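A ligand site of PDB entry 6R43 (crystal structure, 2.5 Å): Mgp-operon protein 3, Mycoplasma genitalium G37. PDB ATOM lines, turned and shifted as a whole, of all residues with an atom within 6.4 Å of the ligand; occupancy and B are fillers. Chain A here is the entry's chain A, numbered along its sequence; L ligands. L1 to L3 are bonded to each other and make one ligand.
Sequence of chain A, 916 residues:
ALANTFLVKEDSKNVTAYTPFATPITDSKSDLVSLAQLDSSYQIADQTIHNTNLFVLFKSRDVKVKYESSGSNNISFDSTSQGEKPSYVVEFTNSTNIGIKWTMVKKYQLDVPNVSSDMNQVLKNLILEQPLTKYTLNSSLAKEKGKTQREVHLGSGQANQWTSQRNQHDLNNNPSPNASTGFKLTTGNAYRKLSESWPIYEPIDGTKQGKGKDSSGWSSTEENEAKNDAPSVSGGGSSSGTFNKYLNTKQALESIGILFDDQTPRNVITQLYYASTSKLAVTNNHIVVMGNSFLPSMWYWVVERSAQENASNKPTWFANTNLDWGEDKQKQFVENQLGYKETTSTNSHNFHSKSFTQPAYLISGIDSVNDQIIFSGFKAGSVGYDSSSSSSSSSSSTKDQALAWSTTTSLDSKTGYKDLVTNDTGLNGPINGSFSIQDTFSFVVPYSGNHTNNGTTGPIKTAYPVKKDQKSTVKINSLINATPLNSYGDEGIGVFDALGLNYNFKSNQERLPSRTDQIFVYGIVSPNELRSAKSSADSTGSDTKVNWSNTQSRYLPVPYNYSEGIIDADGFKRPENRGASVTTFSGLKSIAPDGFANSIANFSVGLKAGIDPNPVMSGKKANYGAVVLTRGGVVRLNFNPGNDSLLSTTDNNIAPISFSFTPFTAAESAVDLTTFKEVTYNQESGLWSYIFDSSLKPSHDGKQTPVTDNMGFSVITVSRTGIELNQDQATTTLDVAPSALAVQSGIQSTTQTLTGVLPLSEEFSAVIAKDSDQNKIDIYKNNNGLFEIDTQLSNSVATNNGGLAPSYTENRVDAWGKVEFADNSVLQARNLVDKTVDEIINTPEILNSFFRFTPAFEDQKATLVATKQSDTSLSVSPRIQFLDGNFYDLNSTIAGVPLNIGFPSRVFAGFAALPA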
ATOM      1  N   ARG A 150     -13.589  -1.347   0.360  1.00  0.00           N
ATOM      2  CA  ARG A 150     -13.579  -0.357  -0.735  1.00  0.00           C
ATOM      3  C   ARG A 150     -12.893  -0.902  -2.002  1.00  0.00           C
ATOM      4  O   ARG A 150     -13.133  -0.299  -3.102  1.00  0.00           O
ATOM      5  CB  ARG A 150     -13.038   0.974  -0.187  1.00  0.00           C
ATOM      6  CG  ARG A 150     -11.610   1.336  -0.575  1.00  0.00           C
ATOM      7  CD  ARG A 150     -11.489   2.365  -1.712  1.00  0.00           C
ATOM      8  NE  ARG A 150     -10.289   2.050  -2.470  1.00  0.00           N
ATOM      9  CZ  ARG A 150      -9.068   1.902  -1.950  1.00  0.00           C
ATOM     10  NH1 ARG A 150      -8.854   2.102  -0.650  1.00  0.00           N
ATOM     11  NH2 ARG A 150      -8.060   1.569  -2.712  1.00  0.00           N
ATOM     12  N   GLN A 158      -9.538   4.245  -5.903  1.00  0.00           N
ATOM     13  CA  GLN A 158      -9.109   5.229  -4.869  1.00  0.00           C
ATOM     14  C   GLN A 158     -10.172   5.389  -3.778  1.00  0.00           C
ATOM     15  O   GLN A 158     -11.371   5.133  -4.054  1.00  0.00           O
ATOM     16  CB  GLN A 158      -8.734   6.554  -5.552  1.00  0.00           C
ATOM     17  CG  GLN A 158      -9.441   6.780  -6.880  1.00  0.00           C
ATOM     18  CD  GLN A 158      -9.470   8.228  -7.304  1.00  0.00           C
ATOM     19  OE1 GLN A 158      -8.434   8.882  -7.416  1.00  0.00           O
ATOM     20  NE2 GLN A 158     -10.664   8.727  -7.559  1.00  0.00           N
ATOM     21  N   ALA A 159      -9.705   5.810  -2.594  1.00  0.00           N
ATOM     22  CA  ALA A 159     -10.490   6.235  -1.404  1.00  0.00           C
ATOM     23  C   ALA A 159     -10.576   7.769  -1.376  1.00  0.00           C
ATOM     24  O   ALA A 159     -10.943   8.349  -0.340  1.00  0.00           O
ATOM     25  CB  ALA A 159      -9.864   5.666  -0.141  1.00  0.00           C
ATOM     26  N   ASN A 160     -10.221   8.395  -2.491  1.00  0.00           N
ATOM     27  CA  ASN A 160     -10.524   9.815  -2.793  1.00  0.00           C
ATOM     28  C   ASN A 160     -11.994   9.897  -3.250  1.00  0.00           C
ATOM     29  O   ASN A 160     -12.584  10.984  -3.133  1.00  0.00           O
ATOM     30  CB  ASN A 160      -9.536  10.353  -3.822  1.00  0.00           C
ATOM     31  CG  ASN A 160      -8.117  10.442  -3.291  1.00  0.00           C
ATOM     32  OD1 ASN A 160      -7.457  11.462  -3.516  1.00  0.00           O
ATOM     33  ND2 ASN A 160      -7.641   9.417  -2.596  1.00  0.00           N
ATOM     34  N   TRP A 162     -14.253   7.463  -2.085  1.00  0.00           N
ATOM     35  CA  TRP A 162     -14.944   6.649  -1.057  1.00  0.00           C
ATOM     36  C   TRP A 162     -16.209   7.346  -0.574  1.00  0.00           C
ATOM     37  O   TRP A 162     -17.206   6.657  -0.294  1.00  0.00           O
ATOM     38  CB  TRP A 162     -14.026   6.344   0.128  1.00  0.00           C
ATOM     39  CG  TRP A 162     -14.704   5.647   1.275  1.00  0.00           C
ATOM     40  CD1 TRP A 162     -14.864   6.135   2.541  1.00  0.00           C
ATOM     41  CD2 TRP A 162     -15.313   4.346   1.273  1.00  0.00           C
ATOM     42  NE1 TRP A 162     -15.528   5.229   3.328  1.00  0.00           N
ATOM     43  CE2 TRP A 162     -15.819   4.114   2.582  1.00  0.00           C
ATOM     44  CE3 TRP A 162     -15.485   3.340   0.305  1.00  0.00           C
ATOM     45  CZ2 TRP A 162     -16.462   2.936   2.939  1.00  0.00           C
ATOM     46  CZ3 TRP A 162     -16.121   2.183   0.657  1.00  0.00           C
ATOM     47  CH2 TRP A 162     -16.601   1.974   1.959  1.00  0.00           C
ATOM     48  N   PRO A 175     -17.152   4.838   7.701  1.00  0.00           N
ATOM     49  CA  PRO A 175     -15.812   5.421   7.803  1.00  0.00           C
ATOM     50  C   PRO A 175     -14.649   4.440   7.585  1.00  0.00           C
ATOM     51  O   PRO A 175     -13.522   4.780   7.925  1.00  0.00           O
ATOM     52  CB  PRO A 175     -15.845   5.924   9.266  1.00  0.00           C
ATOM     53  CG  PRO A 175     -16.640   4.867  10.007  1.00  0.00           C
ATOM     54  CD  PRO A 175     -17.685   4.408   9.013  1.00  0.00           C
ATOM     55  N   SER A 176     -14.917   3.258   7.014  1.00  0.00           N
ATOM     56  CA  SER A 176     -14.037   2.068   7.057  1.00  0.00           C
ATOM     57  C   SER A 176     -13.834   1.490   5.660  1.00  0.00           C
ATOM     58  O   SER A 176     -14.237   0.353   5.384  1.00  0.00           O
ATOM     59  CB  SER A 176     -14.615   1.062   8.009  1.00  0.00           C
ATOM     60  OG  SER A 176     -15.045   1.684   9.208  1.00  0.00           O
ATOM     61  N   PRO A 177     -13.213   2.262   4.741  1.00  0.00           N
ATOM     62  CA  PRO A 177     -12.889   1.764   3.406  1.00  0.00           C
ATOM     63  C   PRO A 177     -11.864   0.625   3.442  1.00  0.00           C
ATOM     64  O   PRO A 177     -11.817  -0.138   2.502  1.00  0.00           O
ATOM     65  CB  PRO A 177     -12.326   2.984   2.670  1.00  0.00           C
ATOM     66  CG  PRO A 177     -11.850   3.914   3.770  1.00  0.00           C
ATOM     67  CD  PRO A 177     -12.794   3.661   4.921  1.00  0.00           C
ATOM     68  N   ASN A 178     -11.086   0.541   4.537  1.00  0.00           N
ATOM     69  CA  ASN A 178      -9.967  -0.422   4.731  1.00  0.00           C
ATOM     70  C   ASN A 178     -10.309  -1.427   5.839  1.00  0.00           C
ATOM     71  O   ASN A 178      -9.377  -2.069   6.412  1.00  0.00           O
ATOM     72  CB  ASN A 178      -8.648   0.306   5.022  1.00  0.00           C
ATOM     73  CG  ASN A 178      -8.479   1.578   4.209  1.00  0.00           C
ATOM     74  OD1 ASN A 178      -8.592   1.560   2.983  1.00  0.00           O
ATOM     75  ND2 ASN A 178      -8.192   2.662   4.900  1.00  0.00           N
ATOM     76  N   ALA A 179     -11.597  -1.551   6.183  1.00  0.00           N
ATOM     77  CA  ALA A 179     -12.091  -2.711   6.960  1.00  0.00           C
ATOM     78  C   ALA A 179     -11.866  -3.938   6.093  1.00  0.00           C
ATOM     79  O   ALA A 179     -11.928  -3.819   4.844  1.00  0.00           O
ATOM     80  CB  ALA A 179     -13.534  -2.567   7.371  1.00  0.00           C
ATOM     81  N   ILE A 431     -16.671  -2.981   9.259  1.00  0.00           N
ATOM     82  CA  ILE A 431     -16.670  -1.654   9.935  1.00  0.00           C
ATOM     83  C   ILE A 431     -15.369  -1.450  10.735  1.00  0.00           C
ATOM     84  O   ILE A 431     -15.078  -0.294  11.092  1.00  0.00           O
ATOM     85  CB  ILE A 431     -17.936  -1.513  10.798  1.00  0.00           C
ATOM     86  CG1 ILE A 431     -18.452  -0.065  10.813  1.00  0.00           C
ATOM     87  CG2 ILE A 431     -17.732  -2.058  12.189  1.00  0.00           C
ATOM     88  CD1 ILE A 431     -19.706   0.148  11.671  1.00  0.00           C
ATOM     89  N   ASN A 432     -14.603  -2.510  11.012  1.00  0.00           N
ATOM     90  CA  ASN A 432     -13.484  -2.526  11.990  1.00  0.00           C
ATOM     91  C   ASN A 432     -12.137  -2.809  11.290  1.00  0.00           C
ATOM     92  O   ASN A 432     -12.063  -3.654  10.333  1.00  0.00           O
ATOM     93  CB  ASN A 432     -13.816  -3.493  13.130  1.00  0.00           C
ATOM     94  CG  ASN A 432     -14.757  -2.896  14.149  1.00  0.00           C
ATOM     95  OD1 ASN A 432     -14.812  -1.667  14.287  1.00  0.00           O
ATOM     96  ND2 ASN A 432     -15.476  -3.737  14.889  1.00  0.00           N
ATOM     97  N   GLY A 433     -11.089  -2.135  11.778  1.00  0.00           N
ATOM     98  CA  GLY A 433      -9.717  -2.237  11.264  1.00  0.00           C
ATOM     99  C   GLY A 433      -8.766  -1.463  12.144  1.00  0.00           C
ATOM    100  O   GLY A 433      -8.402  -2.000  13.175  1.00  0.00           O
ATOM    101  N   SER A 434      -8.407  -0.239  11.760  1.00  0.00           N
ATOM    102  CA  SER A 434      -7.450   0.642  12.494  1.00  0.00           C
ATOM    103  C   SER A 434      -7.850   2.118  12.346  1.00  0.00           C
ATOM    104  O   SER A 434      -8.212   2.538  11.236  1.00  0.00           O
ATOM    105  CB  SER A 434      -6.040   0.383  12.039  1.00  0.00           C
ATOM    106  OG  SER A 434      -5.962   0.491  10.621  1.00  0.00           O
ATOM    107  N   PHE A 435      -7.747   2.863  13.457  1.00  0.00           N
ATOM    108  CA  PHE A 435      -8.306   4.228  13.668  1.00  0.00           C
ATOM    109  C   PHE A 435      -7.383   5.026  14.588  1.00  0.00           C
ATOM    110  O   PHE A 435      -7.345   4.735  15.813  1.00  0.00           O
ATOM    111  CB  PHE A 435      -9.689   4.147  14.313  1.00  0.00           C
ATOM    112  CG  PHE A 435     -10.737   3.424  13.506  1.00  0.00           C
ATOM    113  CD1 PHE A 435     -11.163   3.919  12.296  1.00  0.00           C
ATOM    114  CD2 PHE A 435     -11.324   2.267  13.986  1.00  0.00           C
ATOM    115  CE1 PHE A 435     -12.148   3.269  11.560  1.00  0.00           C
ATOM    116  CE2 PHE A 435     -12.312   1.625  13.238  1.00  0.00           C
ATOM    117  CZ  PHE A 435     -12.718   2.134  12.033  1.00  0.00           C
ATOM    118  N   SER A 436      -6.687   6.031  14.033  1.00  0.00           N
ATOM    119  CA  SER A 436      -5.917   7.052  14.782  1.00  0.00           C
ATOM    120  C   SER A 436      -6.702   8.368  14.794  1.00  0.00           C
ATOM    121  O   SER A 436      -6.474   9.235  13.913  1.00  0.00           O
ATOM    122  CB  SER A 436      -4.527   7.194  14.237  1.00  0.00           C
ATOM    123  OG  SER A 436      -4.508   6.900  12.856  1.00  0.00           O
ATOM    124  N   ILE A 437      -7.646   8.468  15.740  1.00  0.00           N
ATOM    125  CA  ILE A 437      -8.284   9.731  16.238  1.00  0.00           C
ATOM    126  C   ILE A 437      -7.204  10.540  16.983  1.00  0.00           C
ATOM    127  O   ILE A 437      -6.503   9.923  17.815  1.00  0.00           O
ATOM    128  CB  ILE A 437      -9.511   9.433  17.144  1.00  0.00           C
ATOM    129  CG1 ILE A 437      -9.711  10.483  18.250  1.00  0.00           C
ATOM    130  CG2 ILE A 437      -9.482   8.017  17.736  1.00  0.00           C
ATOM    131  CD1 ILE A 437      -9.043  10.170  19.590  1.00  0.00           C
ATOM    132  N   PHE A 441      -4.857   5.404  19.304  1.00  0.00           N
ATOM    133  CA  PHE A 441      -5.069   4.266  18.378  1.00  0.00           C
ATOM    134  C   PHE A 441      -6.225   3.427  18.913  1.00  0.00           C
ATOM    135  O   PHE A 441      -6.451   3.385  20.140  1.00  0.00           O
ATOM    136  CB  PHE A 441      -3.801   3.402  18.206  1.00  0.00           C
ATOM    137  CG  PHE A 441      -3.671   2.673  16.890  1.00  0.00           C
ATOM    138  CD1 PHE A 441      -4.442   1.555  16.613  1.00  0.00           C
ATOM    139  CD2 PHE A 441      -2.736   3.074  15.936  1.00  0.00           C
ATOM    140  CE1 PHE A 441      -4.313   0.876  15.399  1.00  0.00           C
ATOM    141  CE2 PHE A 441      -2.593   2.391  14.742  1.00  0.00           C
ATOM    142  CZ  PHE A 441      -3.389   1.299  14.463  1.00  0.00           C
ATOM    143  N   PHE A 443      -8.699  -0.225  17.166  1.00  0.00           N
ATOM    144  CA  PHE A 443      -9.090  -1.161  16.077  1.00  0.00           C
ATOM    145  C   PHE A 443     -10.585  -1.069  15.806  1.00  0.00           C
ATOM    146  O   PHE A 443     -11.032  -1.404  14.684  1.00  0.00           O
ATOM    147  CB  PHE A 443      -8.743  -2.603  16.451  1.00  0.00           C
ATOM    148  CG  PHE A 443      -7.285  -2.861  16.688  1.00  0.00           C
ATOM    149  CD1 PHE A 443      -6.398  -2.958  15.636  1.00  0.00           C
ATOM    150  CD2 PHE A 443      -6.807  -3.004  17.985  1.00  0.00           C
ATOM    151  CE1 PHE A 443      -5.056  -3.194  15.861  1.00  0.00           C
ATOM    152  CE2 PHE A 443      -5.463  -3.249  18.213  1.00  0.00           C
ATOM    153  CZ  PHE A 443      -4.588  -3.339  17.150  1.00  0.00           C
ATOM    154  N   PRO A 446     -14.848   4.312  16.418  1.00  0.00           N
ATOM    155  CA  PRO A 446     -14.993   5.167  17.598  1.00  0.00           C
ATOM    156  C   PRO A 446     -16.430   5.615  17.875  1.00  0.00           C
ATOM    157  O   PRO A 446     -16.659   6.078  19.000  1.00  0.00           O
ATOM    158  CB  PRO A 446     -14.078   6.365  17.307  1.00  0.00           C
ATOM    159  CG  PRO A 446     -13.309   5.987  16.048  1.00  0.00           C
ATOM    160  CD  PRO A 446     -14.194   5.002  15.306  1.00  0.00           C
ATOM    161  N   TYR A 447     -17.353   5.446  16.910  1.00  0.00           N
ATOM    162  CA  TYR A 447     -18.793   5.848  16.991  1.00  0.00           C
ATOM    163  C   TYR A 447     -19.656   4.965  16.061  1.00  0.00           C
ATOM    164  O   TYR A 447     -19.185   4.634  14.962  1.00  0.00           O
ATOM    165  CB  TYR A 447     -18.977   7.330  16.651  1.00  0.00           C
ATOM    166  CG  TYR A 447     -17.799   7.957  15.951  1.00  0.00           C
ATOM    167  CD1 TYR A 447     -17.356   7.467  14.734  1.00  0.00           C
ATOM    168  CD2 TYR A 447     -17.121   9.023  16.517  1.00  0.00           C
ATOM    169  CE1 TYR A 447     -16.254   8.022  14.089  1.00  0.00           C
ATOM    170  CE2 TYR A 447     -16.029   9.600  15.889  1.00  0.00           C
ATOM    171  CZ  TYR A 447     -15.595   9.099  14.675  1.00  0.00           C
ATOM    172  OH  TYR A 447     -14.531   9.662  14.053  1.00  0.00           O
HETATM  173  C1  LIG L   1      -7.056   6.991   3.147  1.00  0.00           C
HETATM  174  C2  LIG L   1      -6.202   7.142   4.401  1.00  0.00           C
HETATM  175  C3  LIG L   1      -5.218   8.299   4.274  1.00  0.00           C
HETATM  176  C4  LIG L   1      -4.815   8.622   2.815  1.00  0.00           C
HETATM  177  C5  LIG L   1      -3.951   7.521   2.185  1.00  0.00           C
HETATM  178  C6  LIG L   1      -7.252   8.397   2.516  1.00  0.00           C
HETATM  179  O1  LIG L   1      -8.256   8.411   1.493  1.00  0.00           O
HETATM  180  O2  LIG L   1      -8.291   6.319   3.483  1.00  0.00           O
HETATM  181  O3  LIG L   1      -5.461   5.966   4.622  1.00  0.00           O
HETATM  182  O4  LIG L   1      -5.871   9.462   4.795  1.00  0.00           O
HETATM  183  O5  LIG L   1      -5.983   8.908   2.003  1.00  0.00           O
HETATM  184  O6  LIG L   1      -2.810   8.115   1.557  1.00  0.00           O
HETATM  185  C1  LG2 L   2      -5.368   9.967   6.019  1.00  0.00           C
HETATM  186  C2  LG2 L   2      -5.948  11.352   6.240  1.00  0.00           C
HETATM  187  C3  LG2 L   2      -5.017  11.955   7.269  1.00  0.00           C
HETATM  188  C4  LG2 L   2      -5.300  11.211   8.574  1.00  0.00           C
HETATM  189  C5  LG2 L   2      -5.471   9.649   8.428  1.00  0.00           C
HETATM  190  C6  LG2 L   2      -6.591   8.974   9.213  1.00  0.00           C
HETATM  191  O1  LG2 L   2      -6.050  12.145   5.054  1.00  0.00           O
HETATM  192  O2  LG2 L   2      -5.218  13.374   7.324  1.00  0.00           O
HETATM  193  O3  LG2 L   2      -6.438  11.878   9.130  1.00  0.00           O
HETATM  194  O4  LG2 L   2      -5.730   9.122   7.118  1.00  0.00           O
HETATM  195  O5  LG2 L   2      -6.669   7.708   8.544  1.00  0.00           O
HETATM  196  C1  LG3 L   3      -6.990   6.425  10.630  1.00  0.00           C
HETATM  197  C2  LG3 L   3      -7.227   6.525   9.138  1.00  0.00           C
HETATM  198  C3  LG3 L   3      -6.644   5.319   8.378  1.00  0.00           C
HETATM  199  C4  LG3 L   3      -7.454   4.029   8.541  1.00  0.00           C
HETATM  200  C5  LG3 L   3      -8.944   4.210   8.303  1.00  0.00           C
HETATM  201  C6  LG3 L   3      -9.399   5.412   9.101  1.00  0.00           C
HETATM  202  C7  LG3 L   3     -10.850   5.768   8.781  1.00  0.00           C
HETATM  203  C8  LG3 L   3     -11.221   6.923   9.701  1.00  0.00           C
HETATM  204  C9  LG3 L   3     -12.721   6.995   9.938  1.00  0.00           C
HETATM  205  C10 LG3 L   3     -10.423   2.223   8.051  1.00  0.00           C
HETATM  206  C11 LG3 L   3     -11.080   1.106   8.860  1.00  0.00           C
HETATM  207  N1  LG3 L   3      -9.684   3.063   8.789  1.00  0.00           N
HETATM  208  O1  LG3 L   3      -7.787   6.933  11.445  1.00  0.00           O
HETATM  209  O2  LG3 L   3      -5.994   5.838  11.061  1.00  0.00           O
HETATM  210  O3  LG3 L   3      -6.987   3.026   7.641  1.00  0.00           O
HETATM  211  O4  LG3 L   3      -8.616   6.581   8.862  1.00  0.00           O
HETATM  212  O5  LG3 L   3     -11.063   6.127   7.388  1.00  0.00           O
HETATM  213  O6  LG3 L   3     -10.561   6.725  10.946  1.00  0.00           O
HETATM  214  O7  LG3 L   3     -13.060   8.226  10.582  1.00  0.00           O
HETATM  215  O8  LG3 L   3     -10.567   2.318   6.847  1.00  0.00           O
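The backbone NH (N) of Arg 150 is in hydrogen-bond range of the backbone carbonyl oxygen (O) of Pro 177, at 3.0 Å. The side-chain hydroxyl (OG) of Ser 176 sits at hydrogen-bond distance from the backbone carbonyl oxygen (O) of Ile 431, at 2.7 Å.
The backbone NH of Ser 436 is in hydrogen-bond range of an oxygen (O1) of LG3 L3, 3.0 Å away. O2 of LG3 L3 sits at hydrogen-bond distance from OG of Ser 436, 2.6 Å away. The backbone carbonyl oxygen (O) of Pro 175 lies within hydrogen-bond range of an oxygen (O5) of LG3 L3 (2.9 Å). O of Ser 434 lies within hydrogen-bond range of N1 of LG3 L3. An oxygen (O8) of LG3 L3 lies within hydrogen-bond range of the backbone NH (N) of Asn 178 (3.0 Å). The side-chain amide nitrogen of Asn 178 sits at hydrogen-bond distance from an oxygen (O3) of LG3 L3. An oxygen (O1) of LIG L1 is in hydrogen-bond range of the backbone carbonyl oxygen (O) of Ala 159, 3.3 Å away.
The backbone nitrogen of Pro 177 sits close to an oxygen (O8) of LG3 L3 (3.4 Å). CA of Ser 176 touches O8 of LG3 L3, 3.5 Å away. Ala 179 touches the ligand. CD1 of Phe 435 touches O6 of LG3 L3, 3.2 Å away. Hydrophobic or aromatic side chains that line the ligand: Ala 159, Pro 175, Pro 177 and Phe 435. Of the 21 residues printed, 9 come within 4 Å of the ligand. Along chain A the residues within 4 Å of the ligand span positions 159 to 436.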
